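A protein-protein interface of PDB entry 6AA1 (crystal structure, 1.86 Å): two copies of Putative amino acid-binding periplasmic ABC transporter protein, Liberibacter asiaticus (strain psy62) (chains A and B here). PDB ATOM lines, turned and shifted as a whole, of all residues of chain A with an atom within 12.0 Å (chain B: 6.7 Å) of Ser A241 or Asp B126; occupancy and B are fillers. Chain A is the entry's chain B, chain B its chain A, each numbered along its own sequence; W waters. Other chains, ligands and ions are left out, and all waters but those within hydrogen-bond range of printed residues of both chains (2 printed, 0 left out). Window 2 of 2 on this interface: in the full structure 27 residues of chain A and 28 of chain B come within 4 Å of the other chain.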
ATOM      1  N   ASN A 208     -27.662   0.411 -22.527  1.00  0.00           N
ATOM      2  CA  ASN A 208     -26.691   0.894 -21.567  1.00  0.00           C
ATOM      3  C   ASN A 208     -25.718   1.901 -22.160  1.00  0.00           C
ATOM      4  O   ASN A 208     -25.470   2.944 -21.572  1.00  0.00           O
ATOM      5  CB  ASN A 208     -25.938  -0.251 -20.936  1.00  0.00           C
ATOM      6  CG  ASN A 208     -26.800  -1.074 -19.985  1.00  0.00           C
ATOM      7  OD1 ASN A 208     -27.933  -0.690 -19.659  1.00  0.00           O
ATOM      8  ND2 ASN A 208     -26.258  -2.209 -19.523  1.00  0.00           N
ATOM      9  N   GLU A 209     -25.211   1.618 -23.353  1.00  0.00           N
ATOM     10  CA  GLU A 209     -24.259   2.535 -24.018  1.00  0.00           C
ATOM     11  C   GLU A 209     -24.966   3.824 -24.322  1.00  0.00           C
ATOM     12  O   GLU A 209     -24.387   4.875 -24.183  1.00  0.00           O
ATOM     13  CB  GLU A 209     -23.759   1.988 -25.341  1.00  0.00           C
ATOM     14  CG  GLU A 209     -22.922   0.755 -25.249  1.00  0.00           C
ATOM     15  CD  GLU A 209     -22.649   0.140 -26.625  1.00  0.00           C
ATOM     16  OE1 GLU A 209     -22.455   0.910 -27.585  1.00  0.00           O
ATOM     17  OE2 GLU A 209     -22.613  -1.106 -26.724  1.00  0.00           O
ATOM     18  N   ILE A 210     -26.235   3.720 -24.719  1.00  0.00           N
ATOM     19  CA  ILE A 210     -27.015   4.880 -25.081  1.00  0.00           C
ATOM     20  C   ILE A 210     -27.342   5.720 -23.814  1.00  0.00           C
ATOM     21  O   ILE A 210     -27.197   6.956 -23.816  1.00  0.00           O
ATOM     22  CB  ILE A 210     -28.297   4.507 -25.866  1.00  0.00           C
ATOM     23  CG1 ILE A 210     -27.983   3.891 -27.245  1.00  0.00           C
ATOM     24  CG2 ILE A 210     -29.160   5.745 -26.132  1.00  0.00           C
ATOM     25  CD1 ILE A 210     -26.945   4.665 -28.007  1.00  0.00           C
ATOM     26  N   LEU A 211     -27.729   5.047 -22.729  1.00  0.00           N
ATOM     27  CA  LEU A 211     -27.955   5.762 -21.468  1.00  0.00           C
ATOM     28  C   LEU A 211     -26.726   6.580 -20.995  1.00  0.00           C
ATOM     29  O   LEU A 211     -26.845   7.734 -20.560  1.00  0.00           O
ATOM     30  CB  LEU A 211     -28.459   4.812 -20.375  1.00  0.00           C
ATOM     31  CG  LEU A 211     -29.936   4.427 -20.585  1.00  0.00           C
ATOM     32  CD1 LEU A 211     -30.292   3.316 -19.618  1.00  0.00           C
ATOM     33  CD2 LEU A 211     -30.893   5.574 -20.356  1.00  0.00           C
ATOM     34  N   CYS A 212     -25.552   5.983 -21.123  1.00  0.00           N
ATOM     35  CA  CYS A 212     -24.318   6.690 -20.833  1.00  0.00           C
ATOM     36  C   CYS A 212     -24.192   7.942 -21.704  1.00  0.00           C
ATOM     37  O   CYS A 212     -23.868   9.019 -21.214  1.00  0.00           O
ATOM     38  CB  CYS A 212     -23.130   5.757 -21.032  1.00  0.00           C
ATOM     39  SG  CYS A 212     -21.518   6.467 -20.609  1.00  0.00           S
ATOM     40  N   ALA A 213     -24.481   7.802 -22.989  1.00  0.00           N
ATOM     41  CA  ALA A 213     -24.387   8.944 -23.914  1.00  0.00           C
ATOM     42  C   ALA A 213     -25.353  10.098 -23.522  1.00  0.00           C
ATOM     43  O   ALA A 213     -25.043  11.305 -23.559  1.00  0.00           O
ATOM     44  CB  ALA A 213     -24.640   8.454 -25.322  1.00  0.00           C
ATOM     45  N   ILE A 214     -26.561   9.703 -23.149  1.00  0.00           N
ATOM     46  CA  ILE A 214     -27.555  10.643 -22.749  1.00  0.00           C
ATOM     47  C   ILE A 214     -27.131  11.408 -21.467  1.00  0.00           C
ATOM     48  O   ILE A 214     -27.366  12.622 -21.321  1.00  0.00           O
ATOM     49  CB  ILE A 214     -28.872   9.847 -22.624  1.00  0.00           C
ATOM     50  CG1 ILE A 214     -29.390   9.562 -24.036  1.00  0.00           C
ATOM     51  CG2 ILE A 214     -29.915  10.564 -21.777  1.00  0.00           C
ATOM     52  CD1 ILE A 214     -30.576   8.562 -24.062  1.00  0.00           C
ATOM     53  N   HIS A 215     -26.522  10.714 -20.511  1.00  0.00           N
ATOM     54  CA  HIS A 215     -25.993  11.404 -19.376  1.00  0.00           C
ATOM     55  C   HIS A 215     -24.891  12.379 -19.872  1.00  0.00           C
ATOM     56  O   HIS A 215     -24.836  13.534 -19.468  1.00  0.00           O
ATOM     57  CB  HIS A 215     -25.331  10.469 -18.372  1.00  0.00           C
ATOM     58  CG  HIS A 215     -26.283   9.790 -17.442  1.00  0.00           C
ATOM     59  ND1 HIS A 215     -26.781  10.409 -16.312  1.00  0.00           N
ATOM     60  CD2 HIS A 215     -26.815   8.533 -17.463  1.00  0.00           C
ATOM     61  CE1 HIS A 215     -27.597   9.568 -15.693  1.00  0.00           C
ATOM     62  NE2 HIS A 215     -27.657   8.437 -16.385  1.00  0.00           N
ATOM     63  N   LEU A 216     -23.988  11.878 -20.696  1.00  0.00           N
ATOM     64  CA  LEU A 216     -22.812  12.694 -21.015  1.00  0.00           C
ATOM     65  C   LEU A 216     -23.151  13.953 -21.819  1.00  0.00           C
ATOM     66  O   LEU A 216     -22.532  14.991 -21.610  1.00  0.00           O
ATOM     67  CB  LEU A 216     -21.775  11.918 -21.768  1.00  0.00           C
ATOM     68  CG  LEU A 216     -21.041  10.862 -20.976  1.00  0.00           C
ATOM     69  CD1 LEU A 216     -20.446   9.904 -21.971  1.00  0.00           C
ATOM     70  CD2 LEU A 216     -20.006  11.469 -20.039  1.00  0.00           C
ATOM     71  N   ASP A 217     -24.120  13.891 -22.709  1.00  0.00           N
ATOM     72  CA  ASP A 217     -24.422  15.076 -23.475  1.00  0.00           C
ATOM     73  C   ASP A 217     -25.461  16.025 -22.853  1.00  0.00           C
ATOM     74  O   ASP A 217     -25.858  16.976 -23.501  1.00  0.00           O
ATOM     75  CB  ASP A 217     -24.729  14.728 -24.927  1.00  0.00           C
ATOM     76  CG  ASP A 217     -26.102  14.113 -25.142  1.00  0.00           C
ATOM     77  OD1 ASP A 217     -26.996  14.155 -24.267  1.00  0.00           O
ATOM     78  OD2 ASP A 217     -26.299  13.602 -26.254  1.00  0.00           O
ATOM     79  N   GLY A 218     -25.883  15.778 -21.609  1.00  0.00           N
ATOM     80  CA  GLY A 218     -26.864  16.655 -20.944  1.00  0.00           C
ATOM     81  C   GLY A 218     -28.338  16.361 -21.218  1.00  0.00           C
ATOM     82  O   GLY A 218     -29.230  17.019 -20.642  1.00  0.00           O
ATOM     83  N   PRO A 237     -25.994   8.226 -10.630  1.00  0.00           N
ATOM     84  CA  PRO A 237     -24.785   8.854 -11.147  1.00  0.00           C
ATOM     85  C   PRO A 237     -24.730   8.963 -12.663  1.00  0.00           C
ATOM     86  O   PRO A 237     -25.309   8.144 -13.396  1.00  0.00           O
ATOM     87  CB  PRO A 237     -23.633   7.940 -10.658  1.00  0.00           C
ATOM     88  CG  PRO A 237     -24.224   6.955  -9.741  1.00  0.00           C
ATOM     89  CD  PRO A 237     -25.729   7.027  -9.834  1.00  0.00           C
ATOM     90  N   GLY A 238     -23.977   9.975 -13.101  1.00  0.00           N
ATOM     91  CA  GLY A 238     -23.519  10.069 -14.452  1.00  0.00           C
ATOM     92  C   GLY A 238     -22.545   8.975 -14.893  1.00  0.00           C
ATOM     93  O   GLY A 238     -22.320   7.970 -14.186  1.00  0.00           O
ATOM     94  N   CYS A 239     -21.975   9.187 -16.072  1.00  0.00           N
ATOM     95  CA  CYS A 239     -21.020   8.250 -16.648  1.00  0.00           C
ATOM     96  C   CYS A 239     -19.674   8.970 -16.823  1.00  0.00           C
ATOM     97  O   CYS A 239     -19.475  10.057 -16.307  1.00  0.00           O
ATOM     98  CB  CYS A 239     -21.555   7.618 -17.946  1.00  0.00           C
ATOM     99  SG  CYS A 239     -22.922   6.398 -17.727  1.00  0.00           S
ATOM    100  N   SER A 240     -18.696   8.317 -17.408  1.00  0.00           N
ATOM    101  CA  SER A 240     -17.440   8.977 -17.767  1.00  0.00           C
ATOM    102  C   SER A 240     -17.177   8.728 -19.216  1.00  0.00           C
ATOM    103  O   SER A 240     -17.899   7.998 -19.862  1.00  0.00           O
ATOM    104  CB  SER A 240     -16.289   8.424 -16.954  1.00  0.00           C
ATOM    105  OG  SER A 240     -16.410   8.915 -15.649  1.00  0.00           O
ATOM    106  N   SER A 241     -16.142   9.365 -19.741  1.00  0.00           N
ATOM    107  CA  SER A 241     -15.607   9.010 -21.078  1.00  0.00           C
ATOM    108  C   SER A 241     -14.098   8.961 -21.029  1.00  0.00           C
ATOM    109  O   SER A 241     -13.524   9.489 -20.061  1.00  0.00           O
ATOM    110  CB  SER A 241     -16.067  10.044 -22.084  1.00  0.00           C
ATOM    111  OG  SER A 241     -15.775  11.319 -21.565  1.00  0.00           O
ATOM    112  N   ALA B  77     -14.645   2.892 -13.695  1.00  0.00           N
ATOM    113  CA  ALA B  77     -15.660   3.833 -14.129  1.00  0.00           C
ATOM    114  C   ALA B  77     -16.286   3.357 -15.452  1.00  0.00           C
ATOM    115  O   ALA B  77     -15.586   2.989 -16.394  1.00  0.00           O
ATOM    116  CB  ALA B  77     -15.022   5.213 -14.338  1.00  0.00           C
ATOM    117  N   ILE B  78     -17.612   3.443 -15.533  1.00  0.00           N
ATOM    118  CA  ILE B  78     -18.315   3.044 -16.714  1.00  0.00           C
ATOM    119  C   ILE B  78     -18.178   4.161 -17.734  1.00  0.00           C
ATOM    120  O   ILE B  78     -18.372   5.337 -17.398  1.00  0.00           O
ATOM    121  CB  ILE B  78     -19.827   2.834 -16.415  1.00  0.00           C
ATOM    122  CG1 ILE B  78     -20.020   1.607 -15.514  1.00  0.00           C
ATOM    123  CG2 ILE B  78     -20.624   2.612 -17.713  1.00  0.00           C
ATOM    124  CD1 ILE B  78     -21.469   1.420 -15.077  1.00  0.00           C
ATOM    125  N   THR B  79     -17.840   3.776 -18.954  1.00  0.00           N
ATOM    126  CA  THR B  79     -17.742   4.682 -20.116  1.00  0.00           C
ATOM    127  C   THR B  79     -18.359   3.964 -21.333  1.00  0.00           C
ATOM    128  O   THR B  79     -18.414   2.723 -21.398  1.00  0.00           O
ATOM    129  CB  THR B  79     -16.265   5.030 -20.436  1.00  0.00           C
ATOM    130  OG1 THR B  79     -15.639   3.883 -20.955  1.00  0.00           O
ATOM    131  CG2 THR B  79     -15.474   5.423 -19.210  1.00  0.00           C
ATOM    132  N   PRO B  80     -18.830   4.724 -22.316  1.00  0.00           N
ATOM    133  CA  PRO B  80     -19.414   4.081 -23.499  1.00  0.00           C
ATOM    134  C   PRO B  80     -18.444   3.147 -24.234  1.00  0.00           C
ATOM    135  O   PRO B  80     -18.837   2.090 -24.649  1.00  0.00           O
ATOM    136  CB  PRO B  80     -19.753   5.261 -24.412  1.00  0.00           C
ATOM    137  CG  PRO B  80     -19.865   6.427 -23.495  1.00  0.00           C
ATOM    138  CD  PRO B  80     -18.841   6.192 -22.414  1.00  0.00           C
ATOM    139  N   GLU B  81     -17.187   3.524 -24.369  1.00  0.00           N
ATOM    140  CA  GLU B  81     -16.240   2.660 -25.030  1.00  0.00           C
ATOM    141  C   GLU B  81     -16.063   1.350 -24.270  1.00  0.00           C
ATOM    142  O   GLU B  81     -15.960   0.301 -24.877  1.00  0.00           O
ATOM    143  CB  GLU B  81     -14.858   3.305 -25.205  1.00  0.00           C
ATOM    144  CG  GLU B  81     -13.898   2.358 -25.959  1.00  0.00           C
ATOM    145  CD  GLU B  81     -12.393   2.591 -25.703  1.00  0.00           C
ATOM    146  OE1 GLU B  81     -11.758   1.726 -25.028  1.00  0.00           O
ATOM    147  OE2 GLU B  81     -11.833   3.610 -26.201  1.00  0.00           O
ATOM    148  N   ARG B  82     -16.006   1.420 -22.945  1.00  0.00           N
ATOM    149  CA  ARG B  82     -15.901   0.220 -22.160  1.00  0.00           C
ATOM    150  C   ARG B  82     -17.140  -0.648 -22.244  1.00  0.00           C
ATOM    151  O   ARG B  82     -17.014  -1.909 -22.269  1.00  0.00           O
ATOM    152  CB  ARG B  82     -15.593   0.537 -20.689  1.00  0.00           C
ATOM    153  CG  ARG B  82     -14.132   0.890 -20.509  1.00  0.00           C
ATOM    154  CD  ARG B  82     -13.880   1.390 -19.087  1.00  0.00           C
ATOM    155  NE  ARG B  82     -12.538   1.993 -18.973  1.00  0.00           N
ATOM    156  CZ  ARG B  82     -12.165   2.868 -18.049  1.00  0.00           C
ATOM    157  NH1 ARG B  82     -12.969   3.278 -17.081  1.00  0.00           N
ATOM    158  NH2 ARG B  82     -10.937   3.346 -18.091  1.00  0.00           N
ATOM    159  N   ILE B 122      -2.174   9.408 -13.892  1.00  0.00           N
ATOM    160  CA  ILE B 122      -1.775   8.008 -13.857  1.00  0.00           C
ATOM    161  C   ILE B 122      -1.796   7.502 -15.268  1.00  0.00           C
ATOM    162  O   ILE B 122      -2.780   7.639 -15.940  1.00  0.00           O
ATOM    163  CB  ILE B 122      -2.641   7.155 -12.911  1.00  0.00           C
ATOM    164  CG1 ILE B 122      -2.547   7.675 -11.480  1.00  0.00           C
ATOM    165  CG2 ILE B 122      -2.171   5.686 -12.948  1.00  0.00           C
ATOM    166  CD1 ILE B 122      -3.691   7.204 -10.566  1.00  0.00           C
ATOM    167  N   GLY B 124      -2.212   5.257 -18.361  1.00  0.00           N
ATOM    168  CA  GLY B 124      -3.181   4.307 -18.720  1.00  0.00           C
ATOM    169  C   GLY B 124      -4.585   4.654 -18.281  1.00  0.00           C
ATOM    170  O   GLY B 124      -5.432   3.777 -18.387  1.00  0.00           O
ATOM    171  N   THR B 125      -4.870   5.881 -17.802  1.00  0.00           N
ATOM    172  CA  THR B 125      -6.227   6.178 -17.286  1.00  0.00           C
ATOM    173  C   THR B 125      -6.874   7.111 -18.238  1.00  0.00           C
ATOM    174  O   THR B 125      -6.192   7.812 -18.990  1.00  0.00           O
ATOM    175  CB  THR B 125      -6.215   6.842 -15.886  1.00  0.00           C
ATOM    176  OG1 THR B 125      -5.385   8.025 -15.893  1.00  0.00           O
ATOM    177  CG2 THR B 125      -5.690   5.879 -14.860  1.00  0.00           C
ATOM    178  N   ASP B 126      -8.188   7.204 -18.144  1.00  0.00           N
ATOM    179  CA  ASP B 126      -8.928   8.152 -18.936  1.00  0.00           C
ATOM    180  C   ASP B 126      -8.645   9.642 -18.621  1.00  0.00           C
ATOM    181  O   ASP B 126      -8.681  10.484 -19.524  1.00  0.00           O
ATOM    182  CB  ASP B 126     -10.417   7.835 -18.811  1.00  0.00           C
ATOM    183  CG  ASP B 126     -10.821   6.549 -19.615  1.00  0.00           C
ATOM    184  OD1 ASP B 126      -9.965   5.916 -20.302  1.00  0.00           O
ATOM    185  OD2 ASP B 126     -11.997   6.169 -19.537  1.00  0.00           O
ATOM    186  N   LEU B 127      -8.415   9.951 -17.354  1.00  0.00           N
ATOM    187  CA  LEU B 127      -8.002  11.275 -16.927  1.00  0.00           C
ATOM    188  C   LEU B 127      -6.635  11.684 -17.480  1.00  0.00           C
ATOM    189  O   LEU B 127      -6.418  12.876 -17.820  1.00  0.00           O
ATOM    190  CB  LEU B 127      -8.053  11.373 -15.395  1.00  0.00           C
ATOM    191  CG  LEU B 127      -9.469  11.464 -14.836  1.00  0.00           C
ATOM    192  CD1 LEU B 127      -9.312  11.605 -13.325  1.00  0.00           C
ATOM    193  CD2 LEU B 127     -10.223  12.654 -15.456  1.00  0.00           C
ATOM    194  N   SER B 128      -5.709  10.730 -17.636  1.00  0.00           N
ATOM    195  CA  SER B 128      -4.442  11.052 -18.334  1.00  0.00           C
ATOM    196  C   SER B 128      -4.705  11.432 -19.797  1.00  0.00           C
ATOM    197  O   SER B 128      -4.144  12.396 -20.293  1.00  0.00           O
ATOM    198  CB  SER B 128      -3.387   9.938 -18.211  1.00  0.00           C
ATOM    199  OG  SER B 128      -3.643   8.779 -19.008  1.00  0.00           O
ATOM    200  N   ARG B 129      -5.579  10.693 -20.475  1.00  0.00           N
ATOM    201  CA  ARG B 129      -5.952  11.064 -21.848  1.00  0.00           C
ATOM    202  C   ARG B 129      -6.614  12.458 -21.918  1.00  0.00           C
ATOM    203  O   ARG B 129      -6.336  13.226 -22.827  1.00  0.00           O
ATOM    204  CB  ARG B 129      -6.859   9.994 -22.493  1.00  0.00           C
ATOM    205  CG  ARG B 129      -7.108  10.253 -23.978  1.00  0.00           C
ATOM    206  CD  ARG B 129      -7.611   9.019 -24.728  1.00  0.00           C
ATOM    207  NE  ARG B 129      -9.028   8.793 -24.456  1.00  0.00           N
ATOM    208  CZ  ARG B 129      -9.517   7.947 -23.544  1.00  0.00           C
ATOM    209  NH1 ARG B 129      -8.713   7.182 -22.800  1.00  0.00           N
ATOM    210  NH2 ARG B 129     -10.833   7.859 -23.373  1.00  0.00           N
ATOM    211  N   PHE B 130      -7.506  12.785 -20.988  1.00  0.00           N
ATOM    212  CA  PHE B 130      -8.141  14.090 -20.976  1.00  0.00           C
ATOM    213  C   PHE B 130      -7.110  15.213 -20.803  1.00  0.00           C
ATOM    214  O   PHE B 130      -7.139  16.246 -21.496  1.00  0.00           O
ATOM    215  CB  PHE B 130      -9.136  14.091 -19.834  1.00  0.00           C
ATOM    216  CG  PHE B 130      -9.920  15.355 -19.669  1.00  0.00           C
ATOM    217  CD1 PHE B 130     -10.493  15.975 -20.744  1.00  0.00           C
ATOM    218  CD2 PHE B 130     -10.193  15.821 -18.401  1.00  0.00           C
ATOM    219  CE1 PHE B 130     -11.292  17.126 -20.564  1.00  0.00           C
ATOM    220  CE2 PHE B 130     -10.954  16.971 -18.194  1.00  0.00           C
ATOM    221  CZ  PHE B 130     -11.521  17.628 -19.287  1.00  0.00           C
ATOM    222  N   ALA B 131      -6.191  15.007 -19.883  1.00  0.00           N
ATOM    223  CA  ALA B 131      -5.073  15.926 -19.702  1.00  0.00           C
ATOM    224  C   ALA B 131      -4.261  16.132 -20.982  1.00  0.00           C
ATOM    225  O   ALA B 131      -4.023  17.282 -21.388  1.00  0.00           O
ATOM    226  CB  ALA B 131      -4.195  15.458 -18.584  1.00  0.00           C
ATOM    227  N   GLU B 133      -5.432  15.750 -23.952  1.00  0.00           N
ATOM    228  CA  GLU B 133      -6.316  16.416 -24.951  1.00  0.00           C
ATOM    229  C   GLU B 133      -6.443  17.901 -24.671  1.00  0.00           C
ATOM    230  O   GLU B 133      -6.622  18.698 -25.604  1.00  0.00           O
ATOM    231  CB  GLU B 133      -7.695  15.777 -24.968  1.00  0.00           C
ATOM    232  CG  GLU B 133      -7.660  14.347 -25.443  1.00  0.00           C
ATOM    233  CD  GLU B 133      -8.979  13.598 -25.217  1.00  0.00           C
ATOM    234  OE1 GLU B 133      -9.901  14.116 -24.538  1.00  0.00           O
ATOM    235  OE2 GLU B 133      -9.083  12.460 -25.728  1.00  0.00           O
ATOM    236  N   SER B 190     -19.728  10.021 -11.491  1.00  0.00           N
ATOM    237  CA  SER B 190     -19.545   8.948 -12.430  1.00  0.00           C
ATOM    238  C   SER B 190     -19.761   7.643 -11.705  1.00  0.00           C
ATOM    239  O   SER B 190     -19.202   7.430 -10.628  1.00  0.00           O
ATOM    240  CB  SER B 190     -18.113   8.925 -12.997  1.00  0.00           C
ATOM    241  OG  SER B 190     -17.604  10.209 -13.359  1.00  0.00           O
HETATM  242  O   HOH W   1     -15.256  11.344 -14.331  1.00  0.00           O
HETATM  243  O   HOH W   2     -18.841   6.460 -14.996  1.00  0.00           O
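Of the printed residues of chain B, Ser A240 touches Ile B78 (3.0 Å), Thr B79 (3.3 Å), Pro B80 (3.3 Å) and Ser B190 (2.9 Å). Of chain B, only Asp B126 (3.7 Å) comes within 4 Å of Ser A241. No residue of chain A comes within 4 Å of Ala B77. Of the printed residues of chain A, Ile B78 touches Cys A239 and Ser A240. No residue of chain A comes within 4 Å of Gly B124. No residue of chain A comes within 4 Å of Thr B125. Of the printed residues of chain A, Asp B126 touches Ser A241. No residue of chain A comes within 4 Å of Leu B127. No residue of chain A comes within 4 Å of Phe B130. The nearest residue of chain B that does not touch Ser A241 is Thr B79 (4.03 Å). The nearest residue of chain A that does not touch Asp B126 is Ser A240 (5.5 Å).
The side-chain hydroxyl (OG1) of Thr B79 sits at hydrogen-bond distance from the backbone NH (N) of Arg B82 (3.2 Å). The guanidinium group (NH2) of Arg B82 lies within salt-bridge range of the side-chain carboxylate (OD2) of Asp B126. OD1 of Asp B126 is in salt-bridge range of NH1 of Arg B129 (3.1 Å).
No position is printed for both chains. Of the 10 pairs that touch across the chains among the printed residues, none has its exchanged pair printed and touching as well.
The backbone carbonyl oxygen of Ile B78 sits at hydrogen-bond distance from the backbone NH of Ser A240 (3.0 Å). O of Cys A239 lies within hydrogen-bond range of OG of Ser B190 (3.5 Å). The side-chain hydroxyl (OG) of Ser B190 lies within hydrogen-bond range of the side-chain hydroxyl (OG) of Ser A240, 2.9 Å away. The side-chain sulfur (SG) of Cys A212 lies close to the backbone nitrogen (N) of Pro B80 (3.6 Å).
Among the printed residues, no Asp or Glu carboxylate lies within 4 Å of a Lys or Arg side-chain nitrogen of the other chain.
Water W2 bridges the backbone carbonyl oxygen (O) of Ile B78 (2.7 Å) and the backbone NH (N) of Ser A240 (3.0 Å). Water W1 lies within hydrogen-bond range of OG of Ser B190 (2.8 Å) and OG of Ser A240 (3.0 Å).
Pro B80 touches Leu A216. Gly A238 touches Ser B190. Cys A239 touches Ile B78. Ser A240 touches Thr B79 (O to CA, 3.3 Å). Ser A240 touches Pro B80 (O to CD, 3.3 Å). OD2 of Asp B126 touches O of Ser A241, at 3.7 Å.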
